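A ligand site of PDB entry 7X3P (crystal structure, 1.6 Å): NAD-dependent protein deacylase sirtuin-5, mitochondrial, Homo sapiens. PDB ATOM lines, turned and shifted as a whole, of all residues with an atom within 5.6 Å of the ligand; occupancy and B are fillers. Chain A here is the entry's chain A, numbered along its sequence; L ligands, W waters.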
ATOM      1  N   THR A  36      -5.878  -1.206 -30.802  1.00  0.00           N
ATOM      2  CA  THR A  36      -5.774  -2.550 -30.244  1.00  0.00           C
ATOM      3  C   THR A  36      -4.432  -2.826 -29.582  1.00  0.00           C
ATOM      4  O   THR A  36      -4.297  -3.835 -28.899  1.00  0.00           O
ATOM      5  CB  THR A  36      -6.045  -3.584 -31.344  1.00  0.00           C
ATOM      6  OG1 THR A  36      -5.087  -3.432 -32.393  1.00  0.00           O
ATOM      7  CG2 THR A  36      -7.468  -3.397 -31.936  1.00  0.00           C
ATOM      8  N   ARG A  38      -1.598  -3.851 -30.465  1.00  0.00           N
ATOM      9  CA  ARG A  38      -0.948  -5.090 -30.839  1.00  0.00           C
ATOM     10  C   ARG A  38      -0.618  -5.003 -32.315  1.00  0.00           C
ATOM     11  O   ARG A  38      -1.455  -4.570 -33.106  1.00  0.00           O
ATOM     12  CB  ARG A  38      -1.834  -6.316 -30.599  1.00  0.00           C
ATOM     13  CG  ARG A  38      -1.854  -6.807 -29.176  1.00  0.00           C
ATOM     14  CD  ARG A  38      -2.103  -8.301 -29.100  1.00  0.00           C
ATOM     15  NE  ARG A  38      -3.527  -8.601 -29.237  1.00  0.00           N
ATOM     16  CZ  ARG A  38      -4.095  -9.248 -30.248  1.00  0.00           C
ATOM     17  NH1 ARG A  38      -5.396  -9.434 -30.211  1.00  0.00           N
ATOM     18  NH2 ARG A  38      -3.374  -9.723 -31.264  1.00  0.00           N
ATOM     19  N   ALA A  49       0.026  -3.800 -25.617  1.00  0.00           N
ATOM     20  CA  ALA A  49      -0.820  -4.547 -24.686  1.00  0.00           C
ATOM     21  C   ALA A  49      -0.030  -5.588 -23.911  1.00  0.00           C
ATOM     22  O   ALA A  49      -0.252  -5.777 -22.713  1.00  0.00           O
ATOM     23  CB  ALA A  49      -1.976  -5.203 -25.429  1.00  0.00           C
ATOM     24  N   GLN A  50       0.909  -6.274 -24.575  1.00  0.00           N
ATOM     25  CA  GLN A  50       1.603  -7.337 -23.876  1.00  0.00           C
ATOM     26  C   GLN A  50       2.484  -6.840 -22.740  1.00  0.00           C
ATOM     27  O   GLN A  50       2.881  -7.638 -21.889  1.00  0.00           O
ATOM     28  CB  GLN A  50       2.453  -8.159 -24.849  1.00  0.00           C
ATOM     29  CG  GLN A  50       1.660  -9.255 -25.533  1.00  0.00           C
ATOM     30  CD  GLN A  50       2.444 -10.536 -25.694  1.00  0.00           C
ATOM     31  OE1 GLN A  50       2.710 -11.259 -24.715  1.00  0.00           O
ATOM     32  NE2 GLN A  50       2.838 -10.830 -26.923  1.00  0.00           N
ATOM     33  N   ALA A  53      -1.014  -5.606 -20.044  1.00  0.00           N
ATOM     34  CA  ALA A  53      -2.101  -6.553 -19.770  1.00  0.00           C
ATOM     35  C   ALA A  53      -1.534  -7.828 -19.176  1.00  0.00           C
ATOM     36  O   ALA A  53      -1.619  -8.908 -19.762  1.00  0.00           O
ATOM     37  CB  ALA A  53      -2.860  -6.829 -21.058  1.00  0.00           C
ATOM     38  N   PHE A  68      -4.196   3.059 -18.554  1.00  0.00           N
ATOM     39  CA  PHE A  68      -4.284   2.437 -19.867  1.00  0.00           C
ATOM     40  C   PHE A  68      -5.711   2.007 -20.174  1.00  0.00           C
ATOM     41  O   PHE A  68      -6.268   2.336 -21.228  1.00  0.00           O
ATOM     42  CB  PHE A  68      -3.308   1.274 -19.880  1.00  0.00           C
ATOM     43  CG  PHE A  68      -3.293   0.416 -21.131  1.00  0.00           C
ATOM     44  CD1 PHE A  68      -3.090   0.951 -22.383  1.00  0.00           C
ATOM     45  CD2 PHE A  68      -3.398  -0.965 -21.002  1.00  0.00           C
ATOM     46  CE1 PHE A  68      -2.997   0.129 -23.501  1.00  0.00           C
ATOM     47  CE2 PHE A  68      -3.311  -1.780 -22.122  1.00  0.00           C
ATOM     48  CZ  PHE A  68      -3.121  -1.225 -23.359  1.00  0.00           C
ATOM     49  N   TYR A  69      -6.331   1.266 -19.245  1.00  0.00           N
ATOM     50  CA  TYR A  69      -7.694   0.814 -19.522  1.00  0.00           C
ATOM     51  C   TYR A  69      -8.693   1.963 -19.447  1.00  0.00           C
ATOM     52  O   TYR A  69      -9.698   1.937 -20.169  1.00  0.00           O
ATOM     53  CB  TYR A  69      -8.062  -0.329 -18.571  1.00  0.00           C
ATOM     54  CG  TYR A  69      -7.428  -1.619 -19.009  1.00  0.00           C
ATOM     55  CD1 TYR A  69      -7.943  -2.329 -20.075  1.00  0.00           C
ATOM     56  CD2 TYR A  69      -6.298  -2.103 -18.398  1.00  0.00           C
ATOM     57  CE1 TYR A  69      -7.342  -3.484 -20.530  1.00  0.00           C
ATOM     58  CE2 TYR A  69      -5.697  -3.256 -18.843  1.00  0.00           C
ATOM     59  CZ  TYR A  69      -6.208  -3.936 -19.894  1.00  0.00           C
ATOM     60  OH  TYR A  69      -5.598  -5.102 -20.315  1.00  0.00           O
ATOM     61  N   ARG A  72      -8.759   3.511 -22.842  1.00  0.00           N
ATOM     62  CA  ARG A  72      -9.436   2.672 -23.818  1.00  0.00           C
ATOM     63  C   ARG A  72     -10.950   2.699 -23.623  1.00  0.00           C
ATOM     64  O   ARG A  72     -11.690   2.696 -24.603  1.00  0.00           O
ATOM     65  CB  ARG A  72      -8.879   1.259 -23.719  1.00  0.00           C
ATOM     66  CG  ARG A  72      -7.446   1.213 -24.121  1.00  0.00           C
ATOM     67  CD  ARG A  72      -6.824  -0.106 -23.820  1.00  0.00           C
ATOM     68  NE  ARG A  72      -7.336  -1.163 -24.682  1.00  0.00           N
ATOM     69  CZ  ARG A  72      -6.886  -2.404 -24.644  1.00  0.00           C
ATOM     70  NH1 ARG A  72      -7.399  -3.316 -25.470  1.00  0.00           N
ATOM     71  NH2 ARG A  72      -5.964  -2.745 -23.760  1.00  0.00           N
ATOM     72  N   GLN A 107     -12.526 -12.491 -29.236  1.00  0.00           N
ATOM     73  CA  GLN A 107     -11.342 -12.158 -28.473  1.00  0.00           C
ATOM     74  C   GLN A 107     -11.354 -10.712 -27.991  1.00  0.00           C
ATOM     75  O   GLN A 107     -10.536 -10.351 -27.141  1.00  0.00           O
ATOM     76  CB  GLN A 107     -10.085 -12.345 -29.323  1.00  0.00           C
ATOM     77  CG  GLN A 107      -9.863 -13.714 -29.882  1.00  0.00           C
ATOM     78  CD  GLN A 107      -8.721 -13.688 -30.903  1.00  0.00           C
ATOM     79  OE1 GLN A 107      -8.038 -12.658 -31.063  1.00  0.00           O
ATOM     80  NE2 GLN A 107      -8.565 -14.758 -31.634  1.00  0.00           N
ATOM     81  N   ILE A 109     -12.497  -6.998 -26.464  1.00  0.00           N
ATOM     82  CA  ILE A 109     -13.008  -6.547 -25.172  1.00  0.00           C
ATOM     83  C   ILE A 109     -13.752  -5.214 -25.271  1.00  0.00           C
ATOM     84  O   ILE A 109     -14.113  -4.627 -24.255  1.00  0.00           O
ATOM     85  CB  ILE A 109     -11.871  -6.466 -24.132  1.00  0.00           C
ATOM     86  CG1 ILE A 109     -10.787  -5.449 -24.521  1.00  0.00           C
ATOM     87  CG2 ILE A 109     -11.230  -7.836 -23.943  1.00  0.00           C
ATOM     88  CD1 ILE A 109      -9.804  -5.100 -23.370  1.00  0.00           C
ATOM     89  N   HIS A 125     -12.370 -12.982 -23.393  1.00  0.00           N
ATOM     90  CA  HIS A 125     -11.321 -12.259 -22.681  1.00  0.00           C
ATOM     91  C   HIS A 125     -11.880 -11.158 -21.795  1.00  0.00           C
ATOM     92  O   HIS A 125     -11.115 -10.317 -21.323  1.00  0.00           O
ATOM     93  CB  HIS A 125     -10.290 -11.679 -23.658  1.00  0.00           C
ATOM     94  CG  HIS A 125      -9.526 -12.700 -24.439  1.00  0.00           C
ATOM     95  ND1 HIS A 125      -9.173 -12.495 -25.742  1.00  0.00           N
ATOM     96  CD2 HIS A 125      -9.013 -13.911 -24.096  1.00  0.00           C
ATOM     97  CE1 HIS A 125      -8.489 -13.541 -26.189  1.00  0.00           C
ATOM     98  NE2 HIS A 125      -8.373 -14.415 -25.205  1.00  0.00           N
ATOM     99  N   VAL A 187     -10.672  -8.312 -17.488  1.00  0.00           N
ATOM    100  CA  VAL A 187     -10.040  -8.602 -18.769  1.00  0.00           C
ATOM    101  C   VAL A 187      -9.053  -9.731 -18.523  1.00  0.00           C
ATOM    102  O   VAL A 187      -8.332  -9.699 -17.520  1.00  0.00           O
ATOM    103  CB  VAL A 187      -9.333  -7.364 -19.322  1.00  0.00           C
ATOM    104  CG1 VAL A 187      -8.518  -7.707 -20.578  1.00  0.00           C
ATOM    105  CG2 VAL A 187     -10.340  -6.300 -19.680  1.00  0.00           C
ATOM    106  N   VAL A 188      -9.033 -10.733 -19.401  1.00  0.00           N
ATOM    107  CA  VAL A 188      -8.086 -11.828 -19.256  1.00  0.00           C
ATOM    108  C   VAL A 188      -6.726 -11.346 -19.729  1.00  0.00           C
ATOM    109  O   VAL A 188      -6.567 -10.900 -20.867  1.00  0.00           O
ATOM    110  CB  VAL A 188      -8.520 -13.083 -20.034  1.00  0.00           C
ATOM    111  CG1 VAL A 188      -7.492 -14.203 -19.816  1.00  0.00           C
ATOM    112  CG2 VAL A 188      -9.881 -13.563 -19.551  1.00  0.00           C
ATOM    113  N   TRP A 189      -5.743 -11.421 -18.848  1.00  0.00           N
ATOM    114  CA  TRP A 189      -4.415 -10.915 -19.124  1.00  0.00           C
ATOM    115  C   TRP A 189      -3.489 -12.046 -19.535  1.00  0.00           C
ATOM    116  O   TRP A 189      -3.751 -13.229 -19.322  1.00  0.00           O
ATOM    117  CB  TRP A 189      -3.864 -10.213 -17.889  1.00  0.00           C
ATOM    118  CG  TRP A 189      -4.479  -8.872 -17.653  1.00  0.00           C
ATOM    119  CD1 TRP A 189      -5.037  -8.057 -18.592  1.00  0.00           C
ATOM    120  CD2 TRP A 189      -4.606  -8.188 -16.391  1.00  0.00           C
ATOM    121  NE1 TRP A 189      -5.480  -6.897 -18.003  1.00  0.00           N
ATOM    122  CE2 TRP A 189      -5.250  -6.959 -16.646  1.00  0.00           C
ATOM    123  CE3 TRP A 189      -4.248  -8.494 -15.081  1.00  0.00           C
ATOM    124  CZ2 TRP A 189      -5.520  -6.026 -15.645  1.00  0.00           C
ATOM    125  CZ3 TRP A 189      -4.543  -7.577 -14.069  1.00  0.00           C
ATOM    126  CH2 TRP A 189      -5.174  -6.351 -14.374  1.00  0.00           C
ATOM    127  N   PHE A 190      -2.408 -11.663 -20.187  1.00  0.00           N
ATOM    128  CA  PHE A 190      -1.442 -12.659 -20.619  1.00  0.00           C
ATOM    129  C   PHE A 190      -0.890 -13.378 -19.413  1.00  0.00           C
ATOM    130  O   PHE A 190      -0.563 -12.768 -18.384  1.00  0.00           O
ATOM    131  CB  PHE A 190      -0.338 -11.981 -21.444  1.00  0.00           C
ATOM    132  CG  PHE A 190      -0.829 -11.481 -22.759  1.00  0.00           C
ATOM    133  CD1 PHE A 190      -0.942 -12.336 -23.827  1.00  0.00           C
ATOM    134  CD2 PHE A 190      -1.240 -10.178 -22.907  1.00  0.00           C
ATOM    135  CE1 PHE A 190      -1.425 -11.894 -25.038  1.00  0.00           C
ATOM    136  CE2 PHE A 190      -1.751  -9.731 -24.121  1.00  0.00           C
ATOM    137  CZ  PHE A 190      -1.832 -10.597 -25.175  1.00  0.00           C
ATOM    138  N   GLY A 191      -0.822 -14.708 -19.523  1.00  0.00           N
ATOM    139  CA  GLY A 191      -0.448 -15.545 -18.402  1.00  0.00           C
ATOM    140  C   GLY A 191      -1.605 -16.074 -17.577  1.00  0.00           C
ATOM    141  O   GLY A 191      -1.412 -17.002 -16.781  1.00  0.00           O
ATOM    142  N   GLU A 192      -2.788 -15.504 -17.729  1.00  0.00           N
ATOM    143  CA  GLU A 192      -3.975 -15.959 -17.022  1.00  0.00           C
ATOM    144  C   GLU A 192      -4.775 -16.932 -17.892  1.00  0.00           C
ATOM    145  O   GLU A 192      -4.806 -16.799 -19.111  1.00  0.00           O
ATOM    146  CB  GLU A 192      -4.863 -14.779 -16.616  1.00  0.00           C
ATOM    147  CG  GLU A 192      -4.139 -13.799 -15.703  1.00  0.00           C
ATOM    148  CD  GLU A 192      -5.012 -12.635 -15.253  1.00  0.00           C
ATOM    149  OE1 GLU A 192      -5.922 -12.217 -16.006  1.00  0.00           O
ATOM    150  OE2 GLU A 192      -4.757 -12.163 -14.124  1.00  0.00           O
ATOM    151  N   ASN A 193      -5.396 -17.940 -17.302  1.00  0.00           N
ATOM    152  CA  ASN A 193      -6.178 -18.780 -18.185  1.00  0.00           C
ATOM    153  C   ASN A 193      -7.576 -18.178 -18.309  1.00  0.00           C
ATOM    154  O   ASN A 193      -8.012 -17.334 -17.509  1.00  0.00           O
ATOM    155  CB  ASN A 193      -6.245 -20.252 -17.720  1.00  0.00           C
ATOM    156  CG  ASN A 193      -6.680 -21.241 -18.832  1.00  0.00           C
ATOM    157  OD1 ASN A 193      -6.806 -20.896 -20.036  1.00  0.00           O
ATOM    158  ND2 ASN A 193      -6.910 -22.494 -18.430  1.00  0.00           N
ATOM    159  N   LEU A 194      -8.257 -18.591 -19.362  1.00  0.00           N
ATOM    160  CA  LEU A 194      -9.631 -18.225 -19.604  1.00  0.00           C
ATOM    161  C   LEU A 194     -10.506 -18.941 -18.559  1.00  0.00           C
ATOM    162  O   LEU A 194     -10.116 -19.957 -17.975  1.00  0.00           O
ATOM    163  CB  LEU A 194     -10.032 -18.608 -21.027  1.00  0.00           C
ATOM    164  CG  LEU A 194      -9.587 -17.620 -22.127  1.00  0.00           C
ATOM    165  CD1 LEU A 194      -8.083 -17.485 -22.188  1.00  0.00           C
ATOM    166  CD2 LEU A 194     -10.147 -18.083 -23.426  1.00  0.00           C
ATOM    167  N   VAL A 220      -2.578 -15.630 -33.493  1.00  0.00           N
ATOM    168  CA  VAL A 220      -1.383 -15.772 -32.674  1.00  0.00           C
ATOM    169  C   VAL A 220      -1.667 -15.711 -31.180  1.00  0.00           C
ATOM    170  O   VAL A 220      -0.768 -16.076 -30.386  1.00  0.00           O
ATOM    171  CB  VAL A 220      -0.310 -14.720 -33.040  1.00  0.00           C
ATOM    172  CG1 VAL A 220       0.079 -14.861 -34.501  1.00  0.00           C
ATOM    173  CG2 VAL A 220      -0.800 -13.329 -32.751  1.00  0.00           C
ATOM    174  N   VAL A 221      -2.863 -15.318 -30.739  1.00  0.00           N
ATOM    175  CA  VAL A 221      -3.194 -15.284 -29.325  1.00  0.00           C
ATOM    176  C   VAL A 221      -3.864 -16.605 -28.969  1.00  0.00           C
ATOM    177  O   VAL A 221      -4.909 -16.953 -29.523  1.00  0.00           O
ATOM    178  CB  VAL A 221      -4.106 -14.106 -28.962  1.00  0.00           C
ATOM    179  CG1 VAL A 221      -4.533 -14.175 -27.496  1.00  0.00           C
ATOM    180  CG2 VAL A 221      -3.396 -12.803 -29.250  1.00  0.00           C
ATOM    181  N   TYR A 222      -3.254 -17.339 -28.051  1.00  0.00           N
ATOM    182  CA  TYR A 222      -3.735 -18.631 -27.602  1.00  0.00           C
ATOM    183  C   TYR A 222      -4.391 -18.460 -26.230  1.00  0.00           C
ATOM    184  O   TYR A 222      -4.098 -17.517 -25.519  1.00  0.00           O
ATOM    185  CB  TYR A 222      -2.561 -19.637 -27.536  1.00  0.00           C
ATOM    186  CG  TYR A 222      -2.092 -20.083 -28.894  1.00  0.00           C
ATOM    187  CD1 TYR A 222      -1.307 -19.255 -29.672  1.00  0.00           C
ATOM    188  CD2 TYR A 222      -2.453 -21.323 -29.404  1.00  0.00           C
ATOM    189  CE1 TYR A 222      -0.887 -19.658 -30.920  1.00  0.00           C
ATOM    190  CE2 TYR A 222      -2.024 -21.723 -30.662  1.00  0.00           C
ATOM    191  CZ  TYR A 222      -1.254 -20.869 -31.394  1.00  0.00           C
ATOM    192  OH  TYR A 222      -0.834 -21.239 -32.659  1.00  0.00           O
ATOM    193  N   PRO A 223      -5.317 -19.355 -25.891  1.00  0.00           N
ATOM    194  CA  PRO A 223      -5.770 -20.511 -26.668  1.00  0.00           C
ATOM    195  C   PRO A 223      -6.737 -20.227 -27.810  1.00  0.00           C
ATOM    196  O   PRO A 223      -7.052 -21.123 -28.571  1.00  0.00           O
ATOM    197  CB  PRO A 223      -6.461 -21.371 -25.612  1.00  0.00           C
ATOM    198  CG  PRO A 223      -6.988 -20.402 -24.648  1.00  0.00           C
ATOM    199  CD  PRO A 223      -5.942 -19.320 -24.552  1.00  0.00           C
HETATM  200  C1  LIG L   1      -3.053 -19.035 -21.670  1.00  0.00           C
HETATM  201  O1  LIG L   1      -2.752 -19.397 -22.762  1.00  0.00           O
HETATM  202  C2  LIG L   1      -3.002 -19.981 -20.485  1.00  0.00           C
HETATM  203  C3  LIG L   1      -3.259 -21.317 -20.662  1.00  0.00           C
HETATM  204  C4  LIG L   1      -3.189 -22.192 -19.601  1.00  0.00           C
HETATM  205  C5  LIG L   1      -2.872 -21.696 -18.339  1.00  0.00           C
HETATM  206  C6  LIG L   1      -2.622 -20.348 -18.143  1.00  0.00           C
HETATM  207  C7  LIG L   1      -2.679 -19.492 -19.221  1.00  0.00           C
HETATM  208  C8  LIG L   1      -2.760 -22.550 -17.104  1.00  0.00           C
HETATM  209  C9  LIG L   1      -3.068 -24.026 -17.301  1.00  0.00           C
HETATM  210  F1  LIG L   1      -2.942 -24.655 -16.096  1.00  0.00           F
HETATM  211  F2  LIG L   1      -2.249 -24.605 -18.209  1.00  0.00           F
HETATM  212  F3  LIG L   1      -4.337 -24.181 -17.747  1.00  0.00           F
HETATM  213  N1  LIG L   1      -3.039 -22.148 -15.701  1.00  0.00           N
HETATM  214  N2  LIG L   1      -1.784 -22.318 -16.004  1.00  0.00           N
HETATM  215  N3  LIG L   1      -3.422 -17.663 -21.398  1.00  0.00           N
HETATM  216  C10 LIG L   1      -3.423 -16.750 -22.502  1.00  0.00           C
HETATM  217  C11 LIG L   1      -1.977 -16.400 -22.791  1.00  0.00           C
HETATM  218  O2  LIG L   1      -1.162 -16.073 -21.966  1.00  0.00           O
HETATM  219  C12 LIG L   1      -4.219 -15.543 -22.094  1.00  0.00           C
HETATM  220  C13 LIG L   1      -4.276 -14.535 -23.260  1.00  0.00           C
HETATM  221  C14 LIG L   1      -5.205 -13.366 -22.886  1.00  0.00           C
HETATM  222  C15 LIG L   1      -5.250 -12.375 -24.058  1.00  0.00           C
HETATM  223  N4  LIG L   1      -6.089 -11.247 -23.650  1.00  0.00           N
HETATM  224  C16 LIG L   1      -6.579 -10.357 -24.627  1.00  0.00           C
HETATM  225  S1  LIG L   1      -6.141 -10.448 -26.174  1.00  0.00           S
HETATM  226  C17 LIG L   1      -7.613  -9.362 -24.108  1.00  0.00           C
HETATM  227  C18 LIG L   1      -7.184  -7.933 -24.402  1.00  0.00           C
HETATM  228  C19 LIG L   1      -5.867  -7.618 -23.686  1.00  0.00           C
HETATM  229  C20 LIG L   1      -5.733  -6.125 -23.894  1.00  0.00           C
HETATM  230  O3  LIG L   1      -5.741  -5.686 -25.096  1.00  0.00           O
HETATM  231  O4  LIG L   1      -5.713  -5.386 -22.884  1.00  0.00           O
HETATM  232  N5  LIG L   1      -1.580 -16.530 -24.172  1.00  0.00           N
HETATM  233  C21 LIG L   1      -0.215 -16.280 -24.541  1.00  0.00           C
HETATM  234  C22 LIG L   1      -0.197 -15.948 -26.007  1.00  0.00           C
HETATM  235  O5  LIG L   1      -1.002 -16.443 -26.729  1.00  0.00           O
HETATM  236  C23 LIG L   1       0.629 -17.542 -24.385  1.00  0.00           C
HETATM  237  C24 LIG L   1       0.025 -18.788 -24.424  1.00  0.00           C
HETATM  238  C25 LIG L   1       0.796 -19.944 -24.283  1.00  0.00           C
HETATM  239  C26 LIG L   1       2.156 -19.814 -24.101  1.00  0.00           C
HETATM  240  O6  LIG L   1       2.963 -20.968 -23.957  1.00  0.00           O
HETATM  241  C27 LIG L   1       2.768 -18.560 -24.052  1.00  0.00           C
HETATM  242  C28 LIG L   1       1.994 -17.418 -24.191  1.00  0.00           C
HETATM  243  N6  LIG L   1       0.828 -15.044 -26.441  1.00  0.00           N
HETATM  244  C29 LIG L   1       0.908 -14.713 -27.881  1.00  0.00           C
HETATM  245  C30 LIG L   1       0.434 -13.291 -28.178  1.00  0.00           C
HETATM  246  C31 LIG L   1       0.068 -12.183 -28.399  1.00  0.00           C
HETATM  247  O   HOH W   1      -5.984 -22.723 -22.227  1.00  0.00           O
HETATM  248  O   HOH W   2       0.841 -18.090 -20.546  1.00  0.00           O
HETATM  249  O   HOH W   3      -3.322 -23.982 -22.918  1.00  0.00           O
HETATM  250  O   HOH W   4      -5.441  -5.896 -27.572  1.00  0.00           O
HETATM  251  O   HOH W   5      -6.565 -23.670 -15.323  1.00  0.00           O
HETATM  252  O   HOH W   6       2.330 -13.795 -24.217  1.00  0.00           O
HETATM  253  O   HOH W   7      -2.690 -21.805 -24.146  1.00  0.00           O
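OH of Tyr 69 sits at hydrogen-bond distance from O4 of the ligand (2.6 Å). The backbone NH (N) of Tyr 222 is in hydrogen-bond range of an oxygen (O5) of the ligand (2.8 Å). O of Tyr 222 is in hydrogen-bond range of N5 of the ligand, at 3.0 Å. O4 of the ligand lies within salt-bridge range of NH2 of Arg 72 (2.8 Å). N3 of the ligand is in hydrogen-bond range of O of Glu 192. N of Gly 191 sits at hydrogen-bond distance from O2 of the ligand (2.8 Å). A nitrogen (N4) of the ligand sits at hydrogen-bond distance from the backbone carbonyl oxygen (O) of Val 188. A ring nitrogen (ND1) of His 125 sits close to a sulfur (S1) of the ligand (3.7 Å).
NE1 of Trp 189 sits at hydrogen-bond distance from OH of Tyr 69 (2.9 Å). OE1 of Glu 192 sits at hydrogen-bond distance from N of Trp 189, at 3.0 Å. N of Val 188 sits at hydrogen-bond distance from O of His 125, at 2.9 Å. The backbone carbonyl oxygen (O) of Gln 107 lies within hydrogen-bond range of a ring nitrogen (ND1) of His 125, at 2.9 Å. O of Ala 53 sits at hydrogen-bond distance from N of Phe 190 (2.9 Å).
The side-chain amide nitrogen of Asn 193 sits close to a fluorine (F3) of the ligand, 3.2 Å away. Merely in contact with the ligand: Val 220, Gln 50, Val 221, Trp 189, Pro 223, Phe 190, Ala 53, Ala 49 and Ile 109. Hydrophobic or aromatic side chains within 4 Å of the ligand: Ala 49, Ala 53, Tyr 69, Ile 109, His 125, Val 188, Phe 190, Val 221, Tyr 222 and Pro 223. 17 residues have an atom within 4 Å of the ligand: Ala 49, Gln 50, Ala 53, Tyr 69, Arg 72, Ile 109, His 125, Val 188, Trp 189, Phe 190, Gly 191, Glu 192, Asn 193, Val 220, Val 221, Tyr 222 and Pro 223. The nearest printed residue that does not touch the ligand is Val 187 (4.002 Å).
Water W4 bridges O3 of the ligand (2.5 Å) and O of Thr 36 (2.7 Å). Water W6 lies within hydrogen-bond range of the side-chain amide oxygen of Gln 50 (2.6 Å) and a nitrogen (N6) of the ligand (3.0 Å).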
